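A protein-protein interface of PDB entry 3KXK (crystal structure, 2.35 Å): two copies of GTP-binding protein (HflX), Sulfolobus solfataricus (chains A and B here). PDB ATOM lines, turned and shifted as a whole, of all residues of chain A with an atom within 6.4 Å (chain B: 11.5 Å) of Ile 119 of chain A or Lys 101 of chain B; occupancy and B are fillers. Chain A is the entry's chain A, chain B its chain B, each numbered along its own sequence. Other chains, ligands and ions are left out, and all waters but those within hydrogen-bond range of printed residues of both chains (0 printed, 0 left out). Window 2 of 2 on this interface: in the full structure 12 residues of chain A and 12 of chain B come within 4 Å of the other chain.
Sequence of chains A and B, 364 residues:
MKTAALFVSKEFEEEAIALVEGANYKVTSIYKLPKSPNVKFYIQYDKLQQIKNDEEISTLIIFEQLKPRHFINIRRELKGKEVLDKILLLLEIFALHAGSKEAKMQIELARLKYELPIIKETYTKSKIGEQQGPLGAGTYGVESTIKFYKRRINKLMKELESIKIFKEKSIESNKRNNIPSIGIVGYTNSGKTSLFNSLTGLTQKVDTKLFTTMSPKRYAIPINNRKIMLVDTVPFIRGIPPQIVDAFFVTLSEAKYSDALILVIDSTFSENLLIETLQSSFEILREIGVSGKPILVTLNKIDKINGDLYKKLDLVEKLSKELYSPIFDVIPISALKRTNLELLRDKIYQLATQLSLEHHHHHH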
ATOM      1  N   PRO A  68       7.234  -2.637  -1.463  1.00  0.00           N
ATOM      2  CA  PRO A  68       8.373  -3.533  -1.689  1.00  0.00           C
ATOM      3  C   PRO A  68       9.148  -3.116  -2.933  1.00  0.00           C
ATOM      4  O   PRO A  68      10.367  -3.277  -2.990  1.00  0.00           O
ATOM      5  CB  PRO A  68       7.707  -4.893  -1.908  1.00  0.00           C
ATOM      6  CG  PRO A  68       6.422  -4.800  -1.161  1.00  0.00           C
ATOM      7  CD  PRO A  68       5.970  -3.376  -1.300  1.00  0.00           C
ATOM      8  N   ILE A  72      13.368  -2.406  -3.082  1.00  0.00           N
ATOM      9  CA  ILE A  72      14.194  -3.106  -4.057  1.00  0.00           C
ATOM     10  C   ILE A  72      15.015  -2.137  -4.902  1.00  0.00           C
ATOM     11  O   ILE A  72      16.240  -2.231  -4.954  1.00  0.00           O
ATOM     12  CB  ILE A  72      13.337  -3.988  -4.983  1.00  0.00           C
ATOM     13  CG1 ILE A  72      12.640  -5.083  -4.175  1.00  0.00           C
ATOM     14  CG2 ILE A  72      14.193  -4.599  -6.074  1.00  0.00           C
ATOM     15  CD1 ILE A  72      11.761  -5.988  -5.008  1.00  0.00           C
ATOM     16  N   ARG A  75      17.553  -0.087  -2.792  1.00  0.00           N
ATOM     17  CA  ARG A  75      18.644  -0.884  -2.235  1.00  0.00           C
ATOM     18  C   ARG A  75      19.694  -1.272  -3.274  1.00  0.00           C
ATOM     19  O   ARG A  75      20.876  -1.396  -2.949  1.00  0.00           O
ATOM     20  CB  ARG A  75      18.101  -2.130  -1.531  1.00  0.00           C
ATOM     21  CG  ARG A  75      17.508  -1.844  -0.159  1.00  0.00           C
ATOM     22  CD  ARG A  75      16.898  -3.086   0.464  1.00  0.00           C
ATOM     23  NE  ARG A  75      16.421  -2.827   1.820  1.00  0.00           N
ATOM     24  CZ  ARG A  75      15.750  -3.705   2.558  1.00  0.00           C
ATOM     25  NH1 ARG A  75      15.468  -4.906   2.072  1.00  0.00           N
ATOM     26  NH2 ARG A  75      15.357  -3.379   3.782  1.00  0.00           N
ATOM     27  N   TYR A 114       7.915  -8.344   7.306  1.00  0.00           N
ATOM     28  CA  TYR A 114       7.958  -7.197   6.404  1.00  0.00           C
ATOM     29  C   TYR A 114       8.980  -7.418   5.292  1.00  0.00           C
ATOM     30  O   TYR A 114       8.722  -7.115   4.124  1.00  0.00           O
ATOM     31  CB  TYR A 114       8.293  -5.921   7.180  1.00  0.00           C
ATOM     32  CG  TYR A 114       7.865  -4.638   6.501  1.00  0.00           C
ATOM     33  CD1 TYR A 114       6.529  -4.391   6.225  1.00  0.00           C
ATOM     34  CD2 TYR A 114       8.794  -3.664   6.159  1.00  0.00           C
ATOM     35  CE1 TYR A 114       6.128  -3.218   5.610  1.00  0.00           C
ATOM     36  CE2 TYR A 114       8.405  -2.483   5.547  1.00  0.00           C
ATOM     37  CZ  TYR A 114       7.069  -2.263   5.276  1.00  0.00           C
ATOM     38  OH  TYR A 114       6.676  -1.091   4.665  1.00  0.00           O
ATOM     39  N   GLU A 115      10.135  -7.964   5.660  1.00  0.00           N
ATOM     40  CA  GLU A 115      11.199  -8.216   4.695  1.00  0.00           C
ATOM     41  C   GLU A 115      10.854  -9.389   3.785  1.00  0.00           C
ATOM     42  O   GLU A 115      11.381  -9.505   2.677  1.00  0.00           O
ATOM     43  CB  GLU A 115      12.530  -8.466   5.411  1.00  0.00           C
ATOM     44  CG  GLU A 115      13.107  -7.231   6.091  1.00  0.00           C
ATOM     45  CD  GLU A 115      13.640  -6.215   5.100  1.00  0.00           C
ATOM     46  OE1 GLU A 115      13.797  -6.568   3.911  1.00  0.00           O
ATOM     47  OE2 GLU A 115      13.911  -5.067   5.509  1.00  0.00           O
ATOM     48  N   LEU A 116       9.957 -10.253   4.253  1.00  0.00           N
ATOM     49  CA  LEU A 116       9.585 -11.438   3.487  1.00  0.00           C
ATOM     50  C   LEU A 116       8.966 -11.066   2.129  1.00  0.00           C
ATOM     51  O   LEU A 116       9.526 -11.417   1.094  1.00  0.00           O
ATOM     52  CB  LEU A 116       8.686 -12.371   4.307  1.00  0.00           C
ATOM     53  CG  LEU A 116       8.416 -13.773   3.754  1.00  0.00           C
ATOM     54  CD1 LEU A 116       7.261 -13.760   2.765  1.00  0.00           C
ATOM     55  CD2 LEU A 116       9.672 -14.356   3.119  1.00  0.00           C
ATOM     56  N   PRO A 117       7.823 -10.349   2.125  1.00  0.00           N
ATOM     57  CA  PRO A 117       7.312  -9.796   0.864  1.00  0.00           C
ATOM     58  C   PRO A 117       8.360  -9.001   0.096  1.00  0.00           C
ATOM     59  O   PRO A 117       8.446  -9.129  -1.124  1.00  0.00           O
ATOM     60  CB  PRO A 117       6.208  -8.854   1.330  1.00  0.00           C
ATOM     61  CG  PRO A 117       5.688  -9.483   2.553  1.00  0.00           C
ATOM     62  CD  PRO A 117       6.842 -10.189   3.213  1.00  0.00           C
ATOM     63  N   ILE A 118       9.129  -8.177   0.798  1.00  0.00           N
ATOM     64  CA  ILE A 118      10.136  -7.359   0.140  1.00  0.00           C
ATOM     65  C   ILE A 118      11.030  -8.227  -0.731  1.00  0.00           C
ATOM     66  O   ILE A 118      11.120  -8.025  -1.943  1.00  0.00           O
ATOM     67  CB  ILE A 118      11.014  -6.586   1.146  1.00  0.00           C
ATOM     68  CG1 ILE A 118      10.198  -5.508   1.859  1.00  0.00           C
ATOM     69  CG2 ILE A 118      12.198  -5.950   0.426  1.00  0.00           C
ATOM     70  CD1 ILE A 118      11.024  -4.641   2.789  1.00  0.00           C
ATOM     71  N   ILE A 119      11.685  -9.201  -0.108  1.00  0.00           N
ATOM     72  CA  ILE A 119      12.570 -10.099  -0.835  1.00  0.00           C
ATOM     73  C   ILE A 119      11.776 -11.063  -1.712  1.00  0.00           C
ATOM     74  O   ILE A 119      12.277 -11.550  -2.724  1.00  0.00           O
ATOM     75  CB  ILE A 119      13.478 -10.901   0.115  1.00  0.00           C
ATOM     76  CG1 ILE A 119      14.514 -11.689  -0.688  1.00  0.00           C
ATOM     77  CG2 ILE A 119      12.652 -11.830   0.994  1.00  0.00           C
ATOM     78  CD1 ILE A 119      15.413 -12.561   0.153  1.00  0.00           C
ATOM     79  N   LYS A 120      10.533 -11.330  -1.322  1.00  0.00           N
ATOM     80  CA  LYS A 120       9.684 -12.252  -2.065  1.00  0.00           C
ATOM     81  C   LYS A 120       9.263 -11.636  -3.394  1.00  0.00           C
ATOM     82  O   LYS A 120       8.859 -12.342  -4.318  1.00  0.00           O
ATOM     83  CB  LYS A 120       8.450 -12.628  -1.244  1.00  0.00           C
ATOM     84  CG  LYS A 120       7.833 -13.963  -1.616  1.00  0.00           C
ATOM     85  CD  LYS A 120       6.704 -14.320  -0.666  1.00  0.00           C
ATOM     86  CE  LYS A 120       6.233 -15.746  -0.886  1.00  0.00           C
ATOM     87  NZ  LYS A 120       5.799 -15.971  -2.291  1.00  0.00           N
ATOM     88  N   GLU A 121       9.356 -10.313  -3.480  1.00  0.00           N
ATOM     89  CA  GLU A 121       9.064  -9.609  -4.721  1.00  0.00           C
ATOM     90  C   GLU A 121      10.338  -9.488  -5.553  1.00  0.00           C
ATOM     91  O   GLU A 121      10.499  -8.556  -6.339  1.00  0.00           O
ATOM     92  CB  GLU A 121       8.466  -8.228  -4.439  1.00  0.00           C
ATOM     93  CG  GLU A 121       7.929  -7.521  -5.676  1.00  0.00           C
ATOM     94  CD  GLU A 121       7.293  -6.183  -5.360  1.00  0.00           C
ATOM     95  OE1 GLU A 121       6.485  -6.116  -4.410  1.00  0.00           O
ATOM     96  OE2 GLU A 121       7.595  -5.198  -6.067  1.00  0.00           O
ATOM     97  N   THR A 122      11.243 -10.444  -5.367  1.00  0.00           N
ATOM     98  CA  THR A 122      12.488 -10.485  -6.123  1.00  0.00           C
ATOM     99  C   THR A 122      12.548 -11.731  -6.999  1.00  0.00           C
ATOM    100  O   THR A 122      12.731 -11.640  -8.213  1.00  0.00           O
ATOM    101  CB  THR A 122      13.715 -10.467  -5.194  1.00  0.00           C
ATOM    102  OG1 THR A 122      13.797  -9.201  -4.530  1.00  0.00           O
ATOM    103  CG2 THR A 122      14.990 -10.698  -5.989  1.00  0.00           C
ATOM    104  N   PHE B  94      16.523 -27.922   7.823  1.00  0.00           N
ATOM    105  CA  PHE B  94      16.195 -27.031   6.714  1.00  0.00           C
ATOM    106  C   PHE B  94      17.242 -25.933   6.572  1.00  0.00           C
ATOM    107  O   PHE B  94      17.719 -25.654   5.473  1.00  0.00           O
ATOM    108  CB  PHE B  94      14.813 -26.404   6.912  1.00  0.00           C
ATOM    109  CG  PHE B  94      13.674 -27.378   6.782  1.00  0.00           C
ATOM    110  CD1 PHE B  94      13.912 -28.729   6.592  1.00  0.00           C
ATOM    111  CD2 PHE B  94      12.362 -26.937   6.854  1.00  0.00           C
ATOM    112  CE1 PHE B  94      12.862 -29.622   6.475  1.00  0.00           C
ATOM    113  CE2 PHE B  94      11.309 -27.825   6.739  1.00  0.00           C
ATOM    114  CZ  PHE B  94      11.559 -29.170   6.549  1.00  0.00           C
ATOM    115  N   ALA B  95      17.596 -25.314   7.694  1.00  0.00           N
ATOM    116  CA  ALA B  95      18.558 -24.216   7.699  1.00  0.00           C
ATOM    117  C   ALA B  95      19.937 -24.668   7.229  1.00  0.00           C
ATOM    118  O   ALA B  95      20.704 -23.878   6.678  1.00  0.00           O
ATOM    119  CB  ALA B  95      18.643 -23.590   9.084  1.00  0.00           C
ATOM    120  N   LEU B  96      20.250 -25.941   7.454  1.00  0.00           N
ATOM    121  CA  LEU B  96      21.537 -26.493   7.048  1.00  0.00           C
ATOM    122  C   LEU B  96      21.627 -26.652   5.533  1.00  0.00           C
ATOM    123  O   LEU B  96      22.673 -26.400   4.934  1.00  0.00           O
ATOM    124  CB  LEU B  96      21.787 -27.837   7.736  1.00  0.00           C
ATOM    125  CG  LEU B  96      21.873 -27.803   9.264  1.00  0.00           C
ATOM    126  CD1 LEU B  96      22.049 -29.206   9.825  1.00  0.00           C
ATOM    127  CD2 LEU B  96      23.005 -26.894   9.719  1.00  0.00           C
ATOM    128  N   HIS B  97      20.523 -27.068   4.918  1.00  0.00           N
ATOM    129  CA  HIS B  97      20.479 -27.261   3.472  1.00  0.00           C
ATOM    130  C   HIS B  97      20.082 -25.980   2.743  1.00  0.00           C
ATOM    131  O   HIS B  97      20.179 -25.898   1.518  1.00  0.00           O
ATOM    132  CB  HIS B  97      19.514 -28.390   3.110  1.00  0.00           C
ATOM    133  CG  HIS B  97      19.938 -29.734   3.615  1.00  0.00           C
ATOM    134  ND1 HIS B  97      19.646 -30.178   4.886  1.00  0.00           N
ATOM    135  CD2 HIS B  97      20.629 -30.733   3.017  1.00  0.00           C
ATOM    136  CE1 HIS B  97      20.142 -31.392   5.051  1.00  0.00           C
ATOM    137  NE2 HIS B  97      20.744 -31.751   3.930  1.00  0.00           N
ATOM    138  N   ALA B  98      19.636 -24.984   3.501  1.00  0.00           N
ATOM    139  CA  ALA B  98      19.218 -23.711   2.925  1.00  0.00           C
ATOM    140  C   ALA B  98      20.380 -23.012   2.227  1.00  0.00           C
ATOM    141  O   ALA B  98      21.476 -22.911   2.778  1.00  0.00           O
ATOM    142  CB  ALA B  98      18.621 -22.813   3.997  1.00  0.00           C
ATOM    143  N   GLY B  99      20.133 -22.529   1.013  1.00  0.00           N
ATOM    144  CA  GLY B  99      21.155 -21.849   0.240  1.00  0.00           C
ATOM    145  C   GLY B  99      20.752 -20.445  -0.167  1.00  0.00           C
ATOM    146  O   GLY B  99      21.603 -19.615  -0.488  1.00  0.00           O
ATOM    147  N   SER B 100      19.450 -20.177  -0.154  1.00  0.00           N
ATOM    148  CA  SER B 100      18.935 -18.863  -0.521  1.00  0.00           C
ATOM    149  C   SER B 100      18.451 -18.098   0.706  1.00  0.00           C
ATOM    150  O   SER B 100      17.971 -18.695   1.671  1.00  0.00           O
ATOM    151  CB  SER B 100      17.797 -18.996  -1.536  1.00  0.00           C
ATOM    152  OG  SER B 100      16.691 -19.681  -0.976  1.00  0.00           O
ATOM    153  N   LYS B 101      18.579 -16.775   0.665  1.00  0.00           N
ATOM    154  CA  LYS B 101      18.154 -15.930   1.776  1.00  0.00           C
ATOM    155  C   LYS B 101      16.664 -16.091   2.062  1.00  0.00           C
ATOM    156  O   LYS B 101      16.246 -16.124   3.221  1.00  0.00           O
ATOM    157  CB  LYS B 101      18.488 -14.461   1.502  1.00  0.00           C
ATOM    158  CG  LYS B 101      17.941 -13.496   2.544  1.00  0.00           C
ATOM    159  CD  LYS B 101      18.545 -12.109   2.391  1.00  0.00           C
ATOM    160  CE  LYS B 101      20.045 -12.134   2.644  1.00  0.00           C
ATOM    161  NZ  LYS B 101      20.654 -10.777   2.561  1.00  0.00           N
ATOM    162  N   GLU B 102      15.867 -16.192   1.004  1.00  0.00           N
ATOM    163  CA  GLU B 102      14.427 -16.376   1.149  1.00  0.00           C
ATOM    164  C   GLU B 102      14.122 -17.620   1.977  1.00  0.00           C
ATOM    165  O   GLU B 102      13.248 -17.602   2.844  1.00  0.00           O
ATOM    166  CB  GLU B 102      13.753 -16.478  -0.220  1.00  0.00           C
ATOM    167  CG  GLU B 102      12.247 -16.672  -0.153  1.00  0.00           C
ATOM    168  CD  GLU B 102      11.620 -16.835  -1.523  1.00  0.00           C
ATOM    169  OE1 GLU B 102      12.372 -16.905  -2.517  1.00  0.00           O
ATOM    170  OE2 GLU B 102      10.374 -16.894  -1.605  1.00  0.00           O
ATOM    171  N   ALA B 103      14.849 -18.699   1.703  1.00  0.00           N
ATOM    172  CA  ALA B 103      14.684 -19.939   2.450  1.00  0.00           C
ATOM    173  C   ALA B 103      15.052 -19.737   3.915  1.00  0.00           C
ATOM    174  O   ALA B 103      14.327 -20.169   4.810  1.00  0.00           O
ATOM    175  CB  ALA B 103      15.522 -21.048   1.837  1.00  0.00           C
ATOM    176  N   LYS B 104      16.181 -19.075   4.152  1.00  0.00           N
ATOM    177  CA  LYS B 104      16.628 -18.770   5.506  1.00  0.00           C
ATOM    178  C   LYS B 104      15.511 -18.098   6.296  1.00  0.00           C
ATOM    179  O   LYS B 104      15.187 -18.506   7.410  1.00  0.00           O
ATOM    180  CB  LYS B 104      17.849 -17.848   5.476  1.00  0.00           C
ATOM    181  CG  LYS B 104      19.062 -18.407   4.748  1.00  0.00           C
ATOM    182  CD  LYS B 104      19.673 -19.580   5.496  1.00  0.00           C
ATOM    183  CE  LYS B 104      21.088 -19.859   5.012  1.00  0.00           C
ATOM    184  NZ  LYS B 104      21.149 -20.066   3.538  1.00  0.00           N
ATOM    185  N   MET B 105      14.928 -17.062   5.702  1.00  0.00           N
ATOM    186  CA  MET B 105      13.880 -16.284   6.351  1.00  0.00           C
ATOM    187  C   MET B 105      12.643 -17.127   6.640  1.00  0.00           C
ATOM    188  O   MET B 105      12.123 -17.113   7.756  1.00  0.00           O
ATOM    189  CB  MET B 105      13.509 -15.076   5.489  1.00  0.00           C
ATOM    190  CG  MET B 105      14.674 -14.146   5.201  1.00  0.00           C
ATOM    191  SD  MET B 105      14.225 -12.787   4.106  1.00  0.00           S
ATOM    192  CE  MET B 105      12.909 -12.018   5.044  1.00  0.00           C
ATOM    193  N   GLN B 106      12.175 -17.856   5.633  1.00  0.00           N
ATOM    194  CA  GLN B 106      11.009 -18.719   5.789  1.00  0.00           C
ATOM    195  C   GLN B 106      11.205 -19.712   6.929  1.00  0.00           C
ATOM    196  O   GLN B 106      10.296 -19.943   7.727  1.00  0.00           O
ATOM    197  CB  GLN B 106      10.714 -19.467   4.488  1.00  0.00           C
ATOM    198  CG  GLN B 106      10.071 -18.615   3.406  1.00  0.00           C
ATOM    199  CD  GLN B 106       8.620 -18.287   3.708  1.00  0.00           C
ATOM    200  OE1 GLN B 106       8.103 -18.620   4.775  1.00  0.00           O
ATOM    201  NE2 GLN B 106       7.954 -17.632   2.764  1.00  0.00           N
ATOM    202  N   ILE B 107      12.396 -20.296   6.999  1.00  0.00           N
ATOM    203  CA  ILE B 107      12.719 -21.251   8.050  1.00  0.00           C
ATOM    204  C   ILE B 107      12.699 -20.581   9.419  1.00  0.00           C
ATOM    205  O   ILE B 107      12.116 -21.105  10.369  1.00  0.00           O
ATOM    206  CB  ILE B 107      14.097 -21.893   7.816  1.00  0.00           C
ATOM    207  CG1 ILE B 107      14.114 -22.633   6.477  1.00  0.00           C
ATOM    208  CG2 ILE B 107      14.444 -22.839   8.954  1.00  0.00           C
ATOM    209  CD1 ILE B 107      15.490 -23.084   6.047  1.00  0.00           C
ATOM    210  N   GLU B 108      13.337 -19.419   9.513  1.00  0.00           N
ATOM    211  CA  GLU B 108      13.391 -18.675  10.764  1.00  0.00           C
ATOM    212  C   GLU B 108      12.002 -18.197  11.178  1.00  0.00           C
ATOM    213  O   GLU B 108      11.667 -18.188  12.362  1.00  0.00           O
ATOM    214  CB  GLU B 108      14.351 -17.489  10.646  1.00  0.00           C
ATOM    215  CG  GLU B 108      14.512 -16.686  11.928  1.00  0.00           C
ATOM    216  CD  GLU B 108      15.122 -17.494  13.059  1.00  0.00           C
ATOM    217  OE1 GLU B 108      15.579 -18.629  12.808  1.00  0.00           O
ATOM    218  OE2 GLU B 108      15.146 -16.990  14.201  1.00  0.00           O
ATOM    219  N   LEU B 109      11.196 -17.803  10.196  1.00  0.00           N
ATOM    220  CA  LEU B 109       9.822 -17.384  10.451  1.00  0.00           C
ATOM    221  C   LEU B 109       9.032 -18.491  11.137  1.00  0.00           C
ATOM    222  O   LEU B 109       8.361 -18.255  12.143  1.00  0.00           O
ATOM    223  CB  LEU B 109       9.131 -16.981   9.146  1.00  0.00           C
ATOM    224  CG  LEU B 109       9.397 -15.565   8.631  1.00  0.00           C
ATOM    225  CD1 LEU B 109       8.894 -15.404   7.205  1.00  0.00           C
ATOM    226  CD2 LEU B 109       8.752 -14.538   9.550  1.00  0.00           C
ATOM    227  N   ALA B 110       9.115 -19.698  10.588  1.00  0.00           N
ATOM    228  CA  ALA B 110       8.427 -20.847  11.162  1.00  0.00           C
ATOM    229  C   ALA B 110       8.943 -21.145  12.565  1.00  0.00           C
ATOM    230  O   ALA B 110       8.172 -21.500  13.456  1.00  0.00           O
ATOM    231  CB  ALA B 110       8.589 -22.064  10.266  1.00  0.00           C
ATOM    232  N   ARG B 218      27.277 -28.573   0.175  1.00  0.00           N
ATOM    233  CA  ARG B 218      27.420 -28.011  -1.163  1.00  0.00           C
ATOM    234  C   ARG B 218      28.896 -27.959  -1.532  1.00  0.00           C
ATOM    235  O   ARG B 218      29.577 -26.967  -1.275  1.00  0.00           O
ATOM    236  CB  ARG B 218      26.808 -26.611  -1.224  1.00  0.00           C
ATOM    237  CG  ARG B 218      26.945 -25.928  -2.576  1.00  0.00           C
ATOM    238  CD  ARG B 218      26.226 -24.588  -2.598  1.00  0.00           C
ATOM    239  NE  ARG B 218      24.784 -24.736  -2.413  1.00  0.00           N
ATOM    240  CZ  ARG B 218      24.164 -24.626  -1.242  1.00  0.00           C
ATOM    241  NH1 ARG B 218      24.859 -24.361  -0.144  1.00  0.00           N
ATOM    242  NH2 ARG B 218      22.849 -24.778  -1.169  1.00  0.00           N
ATOM    243  N   ASP B 246       5.597 -24.516   4.225  1.00  0.00           N
ATOM    244  CA  ASP B 246       6.145 -23.450   3.393  1.00  0.00           C
ATOM    245  C   ASP B 246       7.669 -23.422   3.453  1.00  0.00           C
ATOM    246  O   ASP B 246       8.337 -23.377   2.422  1.00  0.00           O
ATOM    247  CB  ASP B 246       5.576 -22.091   3.806  1.00  0.00           C
ATOM    248  CG  ASP B 246       4.097 -21.959   3.494  1.00  0.00           C
ATOM    249  OD1 ASP B 246       3.535 -22.884   2.871  1.00  0.00           O
ATOM    250  OD2 ASP B 246       3.498 -20.930   3.869  1.00  0.00           O
ATOM    251  N   ALA B 247       8.210 -23.448   4.666  1.00  0.00           N
ATOM    252  CA  ALA B 247       9.656 -23.433   4.857  1.00  0.00           C
ATOM    253  C   ALA B 247      10.319 -24.583   4.107  1.00  0.00           C
ATOM    254  O   ALA B 247      11.387 -24.418   3.515  1.00  0.00           O
ATOM    255  CB  ALA B 247       9.997 -23.495   6.338  1.00  0.00           C
ATOM    256  N   VAL B 250      10.093 -24.048   0.069  1.00  0.00           N
ATOM    257  CA  VAL B 250      10.981 -22.956  -0.309  1.00  0.00           C
ATOM    258  C   VAL B 250      12.434 -23.427  -0.298  1.00  0.00           C
ATOM    259  O   VAL B 250      13.246 -22.995  -1.116  1.00  0.00           O
ATOM    260  CB  VAL B 250      10.822 -21.743   0.628  1.00  0.00           C
ATOM    261  CG1 VAL B 250      11.838 -20.666   0.280  1.00  0.00           C
ATOM    262  CG2 VAL B 250       9.407 -21.192   0.547  1.00  0.00           C
ATOM    263  N   THR B 251      12.750 -24.323   0.632  1.00  0.00           N
ATOM    264  CA  THR B 251      14.096 -24.869   0.744  1.00  0.00           C
ATOM    265  C   THR B 251      14.366 -25.887  -0.359  1.00  0.00           C
ATOM    266  O   THR B 251      15.437 -25.892  -0.965  1.00  0.00           O
ATOM    267  CB  THR B 251      14.319 -25.538   2.112  1.00  0.00           C
ATOM    268  OG1 THR B 251      14.090 -24.583   3.156  1.00  0.00           O
ATOM    269  CG2 THR B 251      15.739 -26.073   2.221  1.00  0.00           C
ATOM    270  N   LEU B 252      13.386 -26.748  -0.616  1.00  0.00           N
ATOM    271  CA  LEU B 252      13.517 -27.778  -1.638  1.00  0.00           C
ATOM    272  C   LEU B 252      13.521 -27.182  -3.042  1.00  0.00           C
ATOM    273  O   LEU B 252      14.211 -27.678  -3.933  1.00  0.00           O
ATOM    274  CB  LEU B 252      12.394 -28.808  -1.511  1.00  0.00           C
ATOM    275  CG  LEU B 252      12.384 -29.916  -2.566  1.00  0.00           C
ATOM    276  CD1 LEU B 252      13.696 -30.685  -2.549  1.00  0.00           C
ATOM    277  CD2 LEU B 252      11.204 -30.853  -2.355  1.00  0.00           C
ATOM    278  N   SER B 253      12.749 -26.117  -3.233  1.00  0.00           N
ATOM    279  CA  SER B 253      12.635 -25.472  -4.537  1.00  0.00           C
ATOM    280  C   SER B 253      13.981 -24.966  -5.048  1.00  0.00           C
ATOM    281  O   SER B 253      14.114 -24.610  -6.220  1.00  0.00           O
ATOM    282  CB  SER B 253      11.623 -24.324  -4.490  1.00  0.00           C
ATOM    283  OG  SER B 253      10.309 -24.812  -4.280  1.00  0.00           O
ATOM    284  N   GLU B 254      14.975 -24.935  -4.167  1.00  0.00           N
ATOM    285  CA  GLU B 254      16.324 -24.540  -4.556  1.00  0.00           C
ATOM    286  C   GLU B 254      16.908 -25.545  -5.543  1.00  0.00           C
ATOM    287  O   GLU B 254      17.973 -25.319  -6.119  1.00  0.00           O
ATOM    288  CB  GLU B 254      17.227 -24.423  -3.328  1.00  0.00           C
ATOM    289  CG  GLU B 254      16.788 -23.367  -2.326  1.00  0.00           C
ATOM    290  CD  GLU B 254      17.722 -23.270  -1.135  1.00  0.00           C
ATOM    291  OE1 GLU B 254      18.732 -24.005  -1.108  1.00  0.00           O
ATOM    292  OE2 GLU B 254      17.446 -22.459  -0.227  1.00  0.00           O
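The guanidinium group of Arg 75 of chain A lies within salt-bridge range of the side-chain carboxylate of Glu 115 of chain A.
O of Ile 119 of chain A lies close to OG1 of Thr 122 of chain A, at 3.3 Å.
CE of Met 105 of chain B touches C of Glu 115 of chain A, at 3.6 Å.
Leu 116 of chain A touches Met 105 of chain B (N to CE, 3.5 Å).
Leu 116 of chain A touches Gln 106 of chain B (CD2 to NE2, 3.7 Å).
Leu 116 of chain A touches Leu 109 of chain B (CG to CD1, 3.8 Å).
Lys 101 of chain B touches Ile 119 of chain A.
Ile 119 of chain A touches Glu 102 of chain B (CD1 to N, 3.8 Å).
CG2 of Ile 119 of chain A touches SD of Met 105 of chain B, 3.6 Å away.
Lys 120 of chain A touches Glu 102 of chain B.
Of chain B, only Met 105 comes within 4 Å of Glu 115 of chain A.
No residue of chain B comes within 4 Å of Pro 117 of chain A.
No residue of chain B comes within 4 Å of Ile 118 of chain A.
No residue of chain B comes within 4 Å of Thr 122 of chain A.
Of the printed residues of chain B, Lys 120 of chain A touches Glu 102.
Printed residues of chain A within 4 Å of Leu 109 of chain B: Leu 116.
Of the printed residues of chain A, Glu 102 of chain B touches Ile 119 (3.8 Å) and Lys 120 (3.9 Å).
Of the printed residues of chain A, Met 105 of chain B touches Glu 115, Leu 116 and Ile 119.
Printed residues of chain A within 4 Å of Gln 106 of chain B: Leu 116 (3.7 Å).
The nearest printed residue of chain A that does not touch Lys 101 of chain B is Leu 116 of chain A (6.8 Å).
The nearest printed residue of chain A that does not touch Met 105 of chain B is Tyr 114 of chain A (6.1 Å).
Of the 12 printed residues of chain A, 4 touch a printed residue of chain B.
Hydrophobic or aromatic side chains of chain A that line the printed part of chain B: Leu 116 and Ile 119.
Of the 25 printed residues of chain B, 5 touch a printed residue of chain A.
Hydrophobic or aromatic side chains of chain B that line the printed part of chain A: Met 105 and Leu 109.
No position is printed for both chains.
Of the 8 pairs that touch across the chains among the printed residues, none has its exchanged pair printed and touching as well.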
